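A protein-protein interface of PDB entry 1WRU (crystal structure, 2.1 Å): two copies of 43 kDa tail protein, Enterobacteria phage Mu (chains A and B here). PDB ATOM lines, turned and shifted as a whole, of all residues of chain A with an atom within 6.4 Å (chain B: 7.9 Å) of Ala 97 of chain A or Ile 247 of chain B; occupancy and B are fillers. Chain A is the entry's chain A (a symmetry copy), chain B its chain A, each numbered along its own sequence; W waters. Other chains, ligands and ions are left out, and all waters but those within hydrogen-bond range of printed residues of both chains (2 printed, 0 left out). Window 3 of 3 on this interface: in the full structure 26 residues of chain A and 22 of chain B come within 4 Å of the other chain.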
ATOM      1  N   ASP A  92      11.888 -28.377  26.668  1.00  0.00           N
ATOM      2  CA  ASP A  92      12.406 -28.562  25.315  1.00  0.00           C
ATOM      3  C   ASP A  92      11.342 -28.551  24.236  1.00  0.00           C
ATOM      4  O   ASP A  92      11.596 -28.117  23.105  1.00  0.00           O
ATOM      5  CB  ASP A  92      13.215 -29.855  25.240  1.00  0.00           C
ATOM      6  CG  ASP A  92      14.576 -29.698  25.860  1.00  0.00           C
ATOM      7  OD1 ASP A  92      14.916 -28.541  26.190  1.00  0.00           O
ATOM      8  OD2 ASP A  92      15.296 -30.703  26.009  1.00  0.00           O
ATOM      9  N   LEU A  93      10.149 -29.004  24.598  1.00  0.00           N
ATOM     10  CA  LEU A  93       9.018 -29.075  23.675  1.00  0.00           C
ATOM     11  C   LEU A  93       8.529 -27.666  23.367  1.00  0.00           C
ATOM     12  O   LEU A  93       8.062 -27.384  22.266  1.00  0.00           O
ATOM     13  CB  LEU A  93       7.875 -29.890  24.303  1.00  0.00           C
ATOM     14  CG  LEU A  93       8.184 -31.282  24.885  1.00  0.00           C
ATOM     15  CD1 LEU A  93       6.893 -31.917  25.407  1.00  0.00           C
ATOM     16  CD2 LEU A  93       8.823 -32.183  23.818  1.00  0.00           C
ATOM     17  N   ASP A  95      10.520 -24.978  23.595  1.00  0.00           N
ATOM     18  CA  ASP A  95      11.655 -24.363  22.919  1.00  0.00           C
ATOM     19  C   ASP A  95      11.937 -24.852  21.493  1.00  0.00           C
ATOM     20  O   ASP A  95      12.048 -24.054  20.572  1.00  0.00           O
ATOM     21  CB  ASP A  95      12.941 -24.572  23.756  1.00  0.00           C
ATOM     22  CG  ASP A  95      12.968 -23.742  25.067  1.00  0.00           C
ATOM     23  OD1 ASP A  95      11.924 -23.176  25.461  1.00  0.00           O
ATOM     24  OD2 ASP A  95      14.046 -23.663  25.718  1.00  0.00           O
ATOM     25  N   CYS A  96      12.033 -26.167  21.317  1.00  0.00           N
ATOM     26  CA  CYS A  96      12.424 -26.722  20.028  1.00  0.00           C
ATOM     27  C   CYS A  96      11.437 -27.110  18.952  1.00  0.00           C
ATOM     28  O   CYS A  96      10.254 -27.313  19.191  1.00  0.00           O
ATOM     29  CB  CYS A  96      13.356 -27.892  20.286  1.00  0.00           C
ATOM     30  SG  CYS A  96      14.465 -27.544  21.658  1.00  0.00           S
ATOM     31  N   ALA A  97      11.976 -27.214  17.745  1.00  0.00           N
ATOM     32  CA  ALA A  97      11.208 -27.554  16.562  1.00  0.00           C
ATOM     33  C   ALA A  97      10.582 -28.936  16.635  1.00  0.00           C
ATOM     34  O   ALA A  97      11.107 -29.855  17.268  1.00  0.00           O
ATOM     35  CB  ALA A  97      12.098 -27.459  15.327  1.00  0.00           C
ATOM     36  N   ALA A  98       9.432 -29.068  15.992  1.00  0.00           N
ATOM     37  CA  ALA A  98       8.762 -30.344  15.956  1.00  0.00           C
ATOM     38  C   ALA A  98       9.523 -31.064  14.861  1.00  0.00           C
ATOM     39  O   ALA A  98       9.764 -30.496  13.802  1.00  0.00           O
ATOM     40  CB  ALA A  98       7.310 -30.163  15.566  1.00  0.00           C
ATOM     41  N   VAL A  99       9.929 -32.297  15.128  1.00  0.00           N
ATOM     42  CA  VAL A  99      10.660 -33.082  14.146  1.00  0.00           C
ATOM     43  C   VAL A  99      10.101 -34.497  14.143  1.00  0.00           C
ATOM     44  O   VAL A  99       9.858 -35.077  15.196  1.00  0.00           O
ATOM     45  CB  VAL A  99      12.161 -33.153  14.490  1.00  0.00           C
ATOM     46  CG1 VAL A  99      12.906 -33.922  13.407  1.00  0.00           C
ATOM     47  CG2 VAL A  99      12.729 -31.751  14.650  1.00  0.00           C
ATOM     48  N   LEU A 117       6.402 -37.004  18.624  1.00  0.00           N
ATOM     49  CA  LEU A 117       7.038 -35.696  18.744  1.00  0.00           C
ATOM     50  C   LEU A 117       7.918 -35.599  19.979  1.00  0.00           C
ATOM     51  O   LEU A 117       8.993 -35.001  19.941  1.00  0.00           O
ATOM     52  CB  LEU A 117       5.974 -34.603  18.746  1.00  0.00           C
ATOM     53  CG  LEU A 117       5.389 -34.494  17.337  1.00  0.00           C
ATOM     54  CD1 LEU A 117       4.253 -33.519  17.312  1.00  0.00           C
ATOM     55  CD2 LEU A 117       6.486 -34.066  16.377  1.00  0.00           C
ATOM     56  N   TYR A 121      13.068 -35.937  22.385  1.00  0.00           N
ATOM     57  CA  TYR A 121      13.381 -35.087  23.524  1.00  0.00           C
ATOM     58  C   TYR A 121      13.394 -35.898  24.812  1.00  0.00           C
ATOM     59  O   TYR A 121      13.637 -35.366  25.896  1.00  0.00           O
ATOM     60  CB  TYR A 121      12.379 -33.926  23.599  1.00  0.00           C
ATOM     61  CG  TYR A 121      12.467 -33.051  22.367  1.00  0.00           C
ATOM     62  CD1 TYR A 121      11.498 -33.106  21.376  1.00  0.00           C
ATOM     63  CD2 TYR A 121      13.568 -32.223  22.160  1.00  0.00           C
ATOM     64  CE1 TYR A 121      11.615 -32.365  20.206  1.00  0.00           C
ATOM     65  CE2 TYR A 121      13.703 -31.474  20.986  1.00  0.00           C
ATOM     66  CZ  TYR A 121      12.720 -31.551  20.015  1.00  0.00           C
ATOM     67  OH  TYR A 121      12.840 -30.815  18.847  1.00  0.00           O
ATOM     68  N   HIS A 145       5.927 -26.538   8.877  1.00  0.00           N
ATOM     69  CA  HIS A 145       7.254 -25.941   8.777  1.00  0.00           C
ATOM     70  C   HIS A 145       7.809 -25.292  10.048  1.00  0.00           C
ATOM     71  O   HIS A 145       7.300 -24.273  10.512  1.00  0.00           O
ATOM     72  CB  HIS A 145       7.247 -24.896   7.660  1.00  0.00           C
ATOM     73  CG  HIS A 145       6.608 -25.367   6.391  1.00  0.00           C
ATOM     74  ND1 HIS A 145       7.102 -26.422   5.653  1.00  0.00           N
ATOM     75  CD2 HIS A 145       5.514 -24.924   5.726  1.00  0.00           C
ATOM     76  CE1 HIS A 145       6.340 -26.608   4.591  1.00  0.00           C
ATOM     77  NE2 HIS A 145       5.370 -25.713   4.611  1.00  0.00           N
ATOM     78  N   SER A 146       8.852 -25.899  10.605  1.00  0.00           N
ATOM     79  CA  SER A 146       9.539 -25.388  11.794  1.00  0.00           C
ATOM     80  C   SER A 146       8.770 -25.077  13.089  1.00  0.00           C
ATOM     81  O   SER A 146       9.376 -24.575  14.038  1.00  0.00           O
ATOM     82  CB  SER A 146      10.339 -24.135  11.422  1.00  0.00           C
ATOM     83  OG  SER A 146       9.505 -22.990  11.396  1.00  0.00           O
ATOM     84  N   GLU A 147       7.469 -25.353  13.154  1.00  0.00           N
ATOM     85  CA  GLU A 147       6.734 -25.068  14.389  1.00  0.00           C
ATOM     86  C   GLU A 147       7.359 -25.881  15.519  1.00  0.00           C
ATOM     87  O   GLU A 147       8.030 -26.879  15.272  1.00  0.00           O
ATOM     88  CB  GLU A 147       5.244 -25.419  14.243  1.00  0.00           C
ATOM     89  CG  GLU A 147       4.923 -26.903  14.185  1.00  0.00           C
ATOM     90  CD  GLU A 147       3.459 -27.175  13.825  1.00  0.00           C
ATOM     91  OE1 GLU A 147       2.578 -26.400  14.247  1.00  0.00           O
ATOM     92  OE2 GLU A 147       3.185 -28.171  13.127  1.00  0.00           O
ATOM     93  N   THR A 148       7.157 -25.459  16.759  1.00  0.00           N
ATOM     94  CA  THR A 148       7.735 -26.193  17.881  1.00  0.00           C
ATOM     95  C   THR A 148       6.875 -27.405  18.173  1.00  0.00           C
ATOM     96  O   THR A 148       5.772 -27.531  17.638  1.00  0.00           O
ATOM     97  CB  THR A 148       7.779 -25.333  19.145  1.00  0.00           C
ATOM     98  OG1 THR A 148       6.440 -25.007  19.535  1.00  0.00           O
ATOM     99  CG2 THR A 148       8.582 -24.055  18.888  1.00  0.00           C
ATOM    100  N   VAL A 149       7.377 -28.297  19.021  1.00  0.00           N
ATOM    101  CA  VAL A 149       6.599 -29.471  19.378  1.00  0.00           C
ATOM    102  C   VAL A 149       5.337 -28.940  20.050  1.00  0.00           C
ATOM    103  O   VAL A 149       4.212 -29.340  19.714  1.00  0.00           O
ATOM    104  CB  VAL A 149       7.359 -30.390  20.356  1.00  0.00           C
ATOM    105  CG1 VAL A 149       6.417 -31.426  20.933  1.00  0.00           C
ATOM    106  CG2 VAL A 149       8.502 -31.081  19.634  1.00  0.00           C
ATOM    107  N   PHE B 204      20.633 -23.412  21.492  1.00  0.00           N
ATOM    108  CA  PHE B 204      20.191 -24.641  20.865  1.00  0.00           C
ATOM    109  C   PHE B 204      21.349 -25.509  20.418  1.00  0.00           C
ATOM    110  O   PHE B 204      22.419 -25.001  20.120  1.00  0.00           O
ATOM    111  CB  PHE B 204      19.287 -24.319  19.693  1.00  0.00           C
ATOM    112  CG  PHE B 204      18.019 -23.668  20.099  1.00  0.00           C
ATOM    113  CD1 PHE B 204      18.006 -22.329  20.480  1.00  0.00           C
ATOM    114  CD2 PHE B 204      16.840 -24.404  20.158  1.00  0.00           C
ATOM    115  CE1 PHE B 204      16.823 -21.723  20.920  1.00  0.00           C
ATOM    116  CE2 PHE B 204      15.654 -23.813  20.596  1.00  0.00           C
ATOM    117  CZ  PHE B 204      15.646 -22.464  20.978  1.00  0.00           C
ATOM    118  N   GLU B 206      21.492 -27.280  17.692  1.00  0.00           N
ATOM    119  CA  GLU B 206      21.681 -27.120  16.263  1.00  0.00           C
ATOM    120  C   GLU B 206      20.694 -26.138  15.666  1.00  0.00           C
ATOM    121  O   GLU B 206      19.502 -26.149  15.992  1.00  0.00           O
ATOM    122  CB  GLU B 206      21.532 -28.471  15.556  1.00  0.00           C
ATOM    123  CG  GLU B 206      20.131 -29.066  15.642  1.00  0.00           C
ATOM    124  CD  GLU B 206      20.008 -30.412  14.941  1.00  0.00           C
ATOM    125  OE1 GLU B 206      20.699 -31.372  15.357  1.00  0.00           O
ATOM    126  OE2 GLU B 206      19.218 -30.509  13.975  1.00  0.00           O
ATOM    127  N   TYR B 207      21.191 -25.289  14.777  1.00  0.00           N
ATOM    128  CA  TYR B 207      20.339 -24.314  14.121  1.00  0.00           C
ATOM    129  C   TYR B 207      20.285 -24.644  12.632  1.00  0.00           C
ATOM    130  O   TYR B 207      21.318 -24.755  11.977  1.00  0.00           O
ATOM    131  CB  TYR B 207      20.895 -22.906  14.324  1.00  0.00           C
ATOM    132  CG  TYR B 207      21.095 -22.527  15.773  1.00  0.00           C
ATOM    133  CD1 TYR B 207      22.229 -22.944  16.477  1.00  0.00           C
ATOM    134  CD2 TYR B 207      20.152 -21.746  16.439  1.00  0.00           C
ATOM    135  CE1 TYR B 207      22.418 -22.589  17.818  1.00  0.00           C
ATOM    136  CE2 TYR B 207      20.324 -21.382  17.765  1.00  0.00           C
ATOM    137  CZ  TYR B 207      21.453 -21.805  18.454  1.00  0.00           C
ATOM    138  OH  TYR B 207      21.600 -21.463  19.775  1.00  0.00           O
ATOM    139  N   THR B 208      19.086 -24.809  12.092  1.00  0.00           N
ATOM    140  CA  THR B 208      18.978 -25.134  10.682  1.00  0.00           C
ATOM    141  C   THR B 208      18.103 -24.151   9.948  1.00  0.00           C
ATOM    142  O   THR B 208      16.952 -23.941  10.323  1.00  0.00           O
ATOM    143  CB  THR B 208      18.411 -26.541  10.478  1.00  0.00           C
ATOM    144  OG1 THR B 208      19.315 -27.498  11.038  1.00  0.00           O
ATOM    145  CG2 THR B 208      18.223 -26.823   9.002  1.00  0.00           C
ATOM    146  N   VAL B 209      18.656 -23.544   8.904  1.00  0.00           N
ATOM    147  CA  VAL B 209      17.910 -22.573   8.117  1.00  0.00           C
ATOM    148  C   VAL B 209      17.354 -23.226   6.864  1.00  0.00           C
ATOM    149  O   VAL B 209      18.107 -23.663   5.992  1.00  0.00           O
ATOM    150  CB  VAL B 209      18.791 -21.375   7.733  1.00  0.00           C
ATOM    151  CG1 VAL B 209      18.875 -20.405   8.899  1.00  0.00           C
ATOM    152  CG2 VAL B 209      20.176 -21.857   7.372  1.00  0.00           C
ATOM    153  N   LYS B 210      16.024 -23.286   6.811  1.00  0.00           N
ATOM    154  CA  LYS B 210      15.267 -23.889   5.722  1.00  0.00           C
ATOM    155  C   LYS B 210      15.834 -25.246   5.319  1.00  0.00           C
ATOM    156  O   LYS B 210      15.613 -26.248   6.006  1.00  0.00           O
ATOM    157  CB  LYS B 210      15.229 -22.962   4.508  1.00  0.00           C
ATOM    158  CG  LYS B 210      14.251 -23.430   3.455  1.00  0.00           C
ATOM    159  CD  LYS B 210      14.303 -22.575   2.215  1.00  0.00           C
ATOM    160  CE  LYS B 210      13.208 -22.986   1.259  1.00  0.00           C
ATOM    161  NZ  LYS B 210      11.869 -22.853   1.885  1.00  0.00           N
ATOM    162  N   TYR B 243      19.684 -32.742  22.856  1.00  0.00           N
ATOM    163  CA  TYR B 243      19.111 -32.474  21.545  1.00  0.00           C
ATOM    164  C   TYR B 243      18.107 -31.321  21.628  1.00  0.00           C
ATOM    165  O   TYR B 243      17.031 -31.471  22.198  1.00  0.00           O
ATOM    166  CB  TYR B 243      18.413 -33.730  21.011  1.00  0.00           C
ATOM    167  CG  TYR B 243      17.643 -33.513  19.722  1.00  0.00           C
ATOM    168  CD1 TYR B 243      18.298 -33.177  18.537  1.00  0.00           C
ATOM    169  CD2 TYR B 243      16.250 -33.641  19.692  1.00  0.00           C
ATOM    170  CE1 TYR B 243      17.576 -32.973  17.345  1.00  0.00           C
ATOM    171  CE2 TYR B 243      15.522 -33.437  18.518  1.00  0.00           C
ATOM    172  CZ  TYR B 243      16.190 -33.103  17.349  1.00  0.00           C
ATOM    173  OH  TYR B 243      15.464 -32.875  16.202  1.00  0.00           O
ATOM    174  N   ARG B 244      18.479 -30.177  21.055  1.00  0.00           N
ATOM    175  CA  ARG B 244      17.642 -28.979  21.050  1.00  0.00           C
ATOM    176  C   ARG B 244      17.774 -28.274  19.709  1.00  0.00           C
ATOM    177  O   ARG B 244      18.637 -27.419  19.523  1.00  0.00           O
ATOM    178  CB  ARG B 244      18.067 -28.027  22.168  1.00  0.00           C
ATOM    179  CG  ARG B 244      17.520 -28.375  23.533  1.00  0.00           C
ATOM    180  CD  ARG B 244      18.173 -27.551  24.636  1.00  0.00           C
ATOM    181  NE  ARG B 244      17.955 -26.102  24.530  1.00  0.00           N
ATOM    182  CZ  ARG B 244      16.783 -25.495  24.682  1.00  0.00           C
ATOM    183  NH1 ARG B 244      15.690 -26.198  24.948  1.00  0.00           N
ATOM    184  NH2 ARG B 244      16.705 -24.172  24.583  1.00  0.00           N
ATOM    185  N   PRO B 245      16.926 -28.642  18.747  1.00  0.00           N
ATOM    186  CA  PRO B 245      16.979 -28.018  17.424  1.00  0.00           C
ATOM    187  C   PRO B 245      16.095 -26.785  17.265  1.00  0.00           C
ATOM    188  O   PRO B 245      15.031 -26.669  17.880  1.00  0.00           O
ATOM    189  CB  PRO B 245      16.515 -29.138  16.513  1.00  0.00           C
ATOM    190  CG  PRO B 245      15.423 -29.755  17.353  1.00  0.00           C
ATOM    191  CD  PRO B 245      16.088 -29.855  18.718  1.00  0.00           C
ATOM    192  N   MET B 246      16.541 -25.887  16.397  1.00  0.00           N
ATOM    193  CA  MET B 246      15.812 -24.667  16.072  1.00  0.00           C
ATOM    194  C   MET B 246      15.841 -24.550  14.552  1.00  0.00           C
ATOM    195  O   MET B 246      16.905 -24.574  13.942  1.00  0.00           O
ATOM    196  CB  MET B 246      16.485 -23.434  16.673  1.00  0.00           C
ATOM    197  CG  MET B 246      16.088 -22.156  15.954  1.00  0.00           C
ATOM    198  SD  MET B 246      16.596 -20.626  16.782  1.00  0.00           S
ATOM    199  CE  MET B 246      15.229 -20.443  17.982  1.00  0.00           C
ATOM    200  N   ILE B 247      14.676 -24.437  13.938  1.00  0.00           N
ATOM    201  CA  ILE B 247      14.626 -24.319  12.499  1.00  0.00           C
ATOM    202  C   ILE B 247      14.273 -22.899  12.115  1.00  0.00           C
ATOM    203  O   ILE B 247      13.365 -22.299  12.686  1.00  0.00           O
ATOM    204  CB  ILE B 247      13.597 -25.289  11.904  1.00  0.00           C
ATOM    205  CG1 ILE B 247      14.111 -26.725  12.045  1.00  0.00           C
ATOM    206  CG2 ILE B 247      13.330 -24.935  10.459  1.00  0.00           C
ATOM    207  CD1 ILE B 247      13.168 -27.787  11.508  1.00  0.00           C
ATOM    208  N   ILE B 248      15.014 -22.366  11.149  1.00  0.00           N
ATOM    209  CA  ILE B 248      14.815 -21.011  10.643  1.00  0.00           C
ATOM    210  C   ILE B 248      14.366 -21.078   9.179  1.00  0.00           C
ATOM    211  O   ILE B 248      15.122 -21.522   8.324  1.00  0.00           O
ATOM    212  CB  ILE B 248      16.125 -20.214  10.717  1.00  0.00           C
ATOM    213  CG1 ILE B 248      16.650 -20.209  12.159  1.00  0.00           C
ATOM    214  CG2 ILE B 248      15.898 -18.804  10.202  1.00  0.00           C
ATOM    215  CD1 ILE B 248      18.055 -19.646  12.316  1.00  0.00           C
ATOM    216  N   ILE B 249      13.142 -20.639   8.894  1.00  0.00           N
ATOM    217  CA  ILE B 249      12.624 -20.672   7.524  1.00  0.00           C
ATOM    218  C   ILE B 249      13.216 -19.557   6.669  1.00  0.00           C
ATOM    219  O   ILE B 249      13.073 -18.378   6.988  1.00  0.00           O
ATOM    220  CB  ILE B 249      11.085 -20.543   7.498  1.00  0.00           C
ATOM    221  CG1 ILE B 249      10.446 -21.742   8.198  1.00  0.00           C
ATOM    222  CG2 ILE B 249      10.596 -20.463   6.060  1.00  0.00           C
ATOM    223  CD1 ILE B 249       8.929 -21.677   8.261  1.00  0.00           C
ATOM    224  N   ALA B 250      13.869 -19.936   5.572  1.00  0.00           N
ATOM    225  CA  ALA B 250      14.488 -18.956   4.689  1.00  0.00           C
ATOM    226  C   ALA B 250      14.000 -19.047   3.251  1.00  0.00           C
ATOM    227  O   ALA B 250      13.282 -19.978   2.879  1.00  0.00           O
ATOM    228  CB  ALA B 250      15.998 -19.112   4.728  1.00  0.00           C
ATOM    229  N   GLU B 266      23.042 -16.935  14.018  1.00  0.00           N
ATOM    230  CA  GLU B 266      22.080 -17.271  15.055  1.00  0.00           C
ATOM    231  C   GLU B 266      22.739 -17.885  16.278  1.00  0.00           C
ATOM    232  O   GLU B 266      22.438 -17.514  17.413  1.00  0.00           O
ATOM    233  CB  GLU B 266      21.046 -18.244  14.483  1.00  0.00           C
ATOM    234  CG  GLU B 266      19.724 -18.247  15.213  1.00  0.00           C
ATOM    235  CD  GLU B 266      19.165 -16.844  15.379  1.00  0.00           C
ATOM    236  OE1 GLU B 266      19.255 -16.046  14.420  1.00  0.00           O
ATOM    237  OE2 GLU B 266      18.630 -16.544  16.468  1.00  0.00           O
HETATM  238  O   HOH W   1      12.183 -24.228  15.722  1.00  0.00           O
HETATM  239  O   HOH W   2      16.567 -32.658  24.590  1.00  0.00           O
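Of the 15 printed residues of chain B, 6 touch a printed residue of chain A. Hydrophobic or aromatic side chains of chain B that line the printed part of chain A: Phe 204, Tyr 243, Pro 245, Ile 247 and Ile 249. Along chain B the printed residues that touch a printed residue of chain A span positions 204 to 249. Of the 14 printed residues of chain A, 8 touch a printed residue of chain B. Hydrophobic or aromatic side chains of chain A that line the printed part of chain B: Ala 97, Val 99, Tyr 121 and His 145. Among the printed residues, Asp or Glu carboxylates within 4 Å of a Lys or Arg side-chain nitrogen of the other chain: Asp 92 of chain A with Arg 244 of chain B and Asp 95 of chain A with Arg 244 of chain B.
Of chain B, only Pro 245 (3.1 Å) and Ile 247 (3.9 Å) come within 4 Å of Ala 97 of chain A. Of chain A, only Ala 97 (3.9 Å) and Ser 146 (3.2 Å) come within 4 Å of Ile 247 of chain B. No residue of chain B comes within 4 Å of Ala 98 of chain A. Of the printed residues of chain B, His 145 of chain A touches Ile 249. Of the printed residues of chain B, Ser 146 of chain A touches Ile 247 (3.2 Å) and Ile 249 (3.4 Å). Of the printed residues of chain A, Ile 249 of chain B touches His 145 (3.7 Å) and Ser 146 (3.4 Å). Printed residues of chain B within 4 Å of Cys 96 of chain A: Arg 244 (3.5 Å) and Pro 245 (3.2 Å). Printed residues of chain A within 4 Å of Pro 245 of chain B: Cys 96, Ala 97 and Tyr 121. The nearest printed residue of chain B that does not touch Asp 92 of chain A is Tyr 243 of chain B (4.3 Å).
The guanidinium group of Arg 244 of chain B lies within salt-bridge range of the side-chain carboxylate of Asp 95 of chain A. The guanidinium group (NH1) of Arg 244 of chain B sits close to the side-chain sulfur (SG) of Cys 96 of chain A. The side-chain carboxylate (OD1) of Asp 92 of chain A is in salt-bridge range of the guanidinium group (NH1) of Arg 244 of chain B, 2.8 Å away. O of Pro 245 of chain B is in hydrogen-bond range of N of Ala 97 of chain A, 3.1 Å away.
O of Ala 97 of chain A lies within hydrogen-bond range of OH of Tyr 121 of chain A. The side-chain hydroxyl (OH) of Tyr 207 of chain B sits at hydrogen-bond distance from the backbone NH (N) of Phe 204 of chain B, at 2.8 Å. SG of Cys 96 of chain A is in hydrogen-bond range of O of Asp 92 of chain A, 3.3 Å away. The backbone NH of Glu 206 of chain B lies within hydrogen-bond range of the backbone carbonyl oxygen of Arg 244 of chain B (3.4 Å). The backbone carbonyl oxygen of Cys 96 of chain A lies within hydrogen-bond range of the backbone NH of Val 149 of chain A (3.0 Å).
Among the printed residues, pairs that only touch across the chains: Asp 95 of chain A with Phe 204 of chain B, Cys 96 of chain A with Pro 245 of chain B, Ala 97 of chain A with Ile 247 of chain B, Val 99 of chain A with Tyr 243 of chain B, Tyr 121 of chain A with Tyr 243 of chain B, Tyr 121 of chain A with Pro 245 of chain B, His 145 of chain A with Ile 249 of chain B, Ser 146 of chain A with Ile 247 of chain B and Ser 146 of chain A with Ile 249 of chain B.
Water W2 lies within hydrogen-bond range of O of Tyr 243 of chain B (2.7 Å) and OD2 of Asp 92 of chain A (2.7 Å). Water W1 lies within hydrogen-bond range of the backbone NH of Ile 247 of chain B (3.1 Å) and the backbone carbonyl oxygen of Ser 146 of chain A (3.3 Å).
No position is printed for both chains. Of the 13 pairs that touch across the chains among the printed residues, none has its exchanged pair printed and touching as well.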
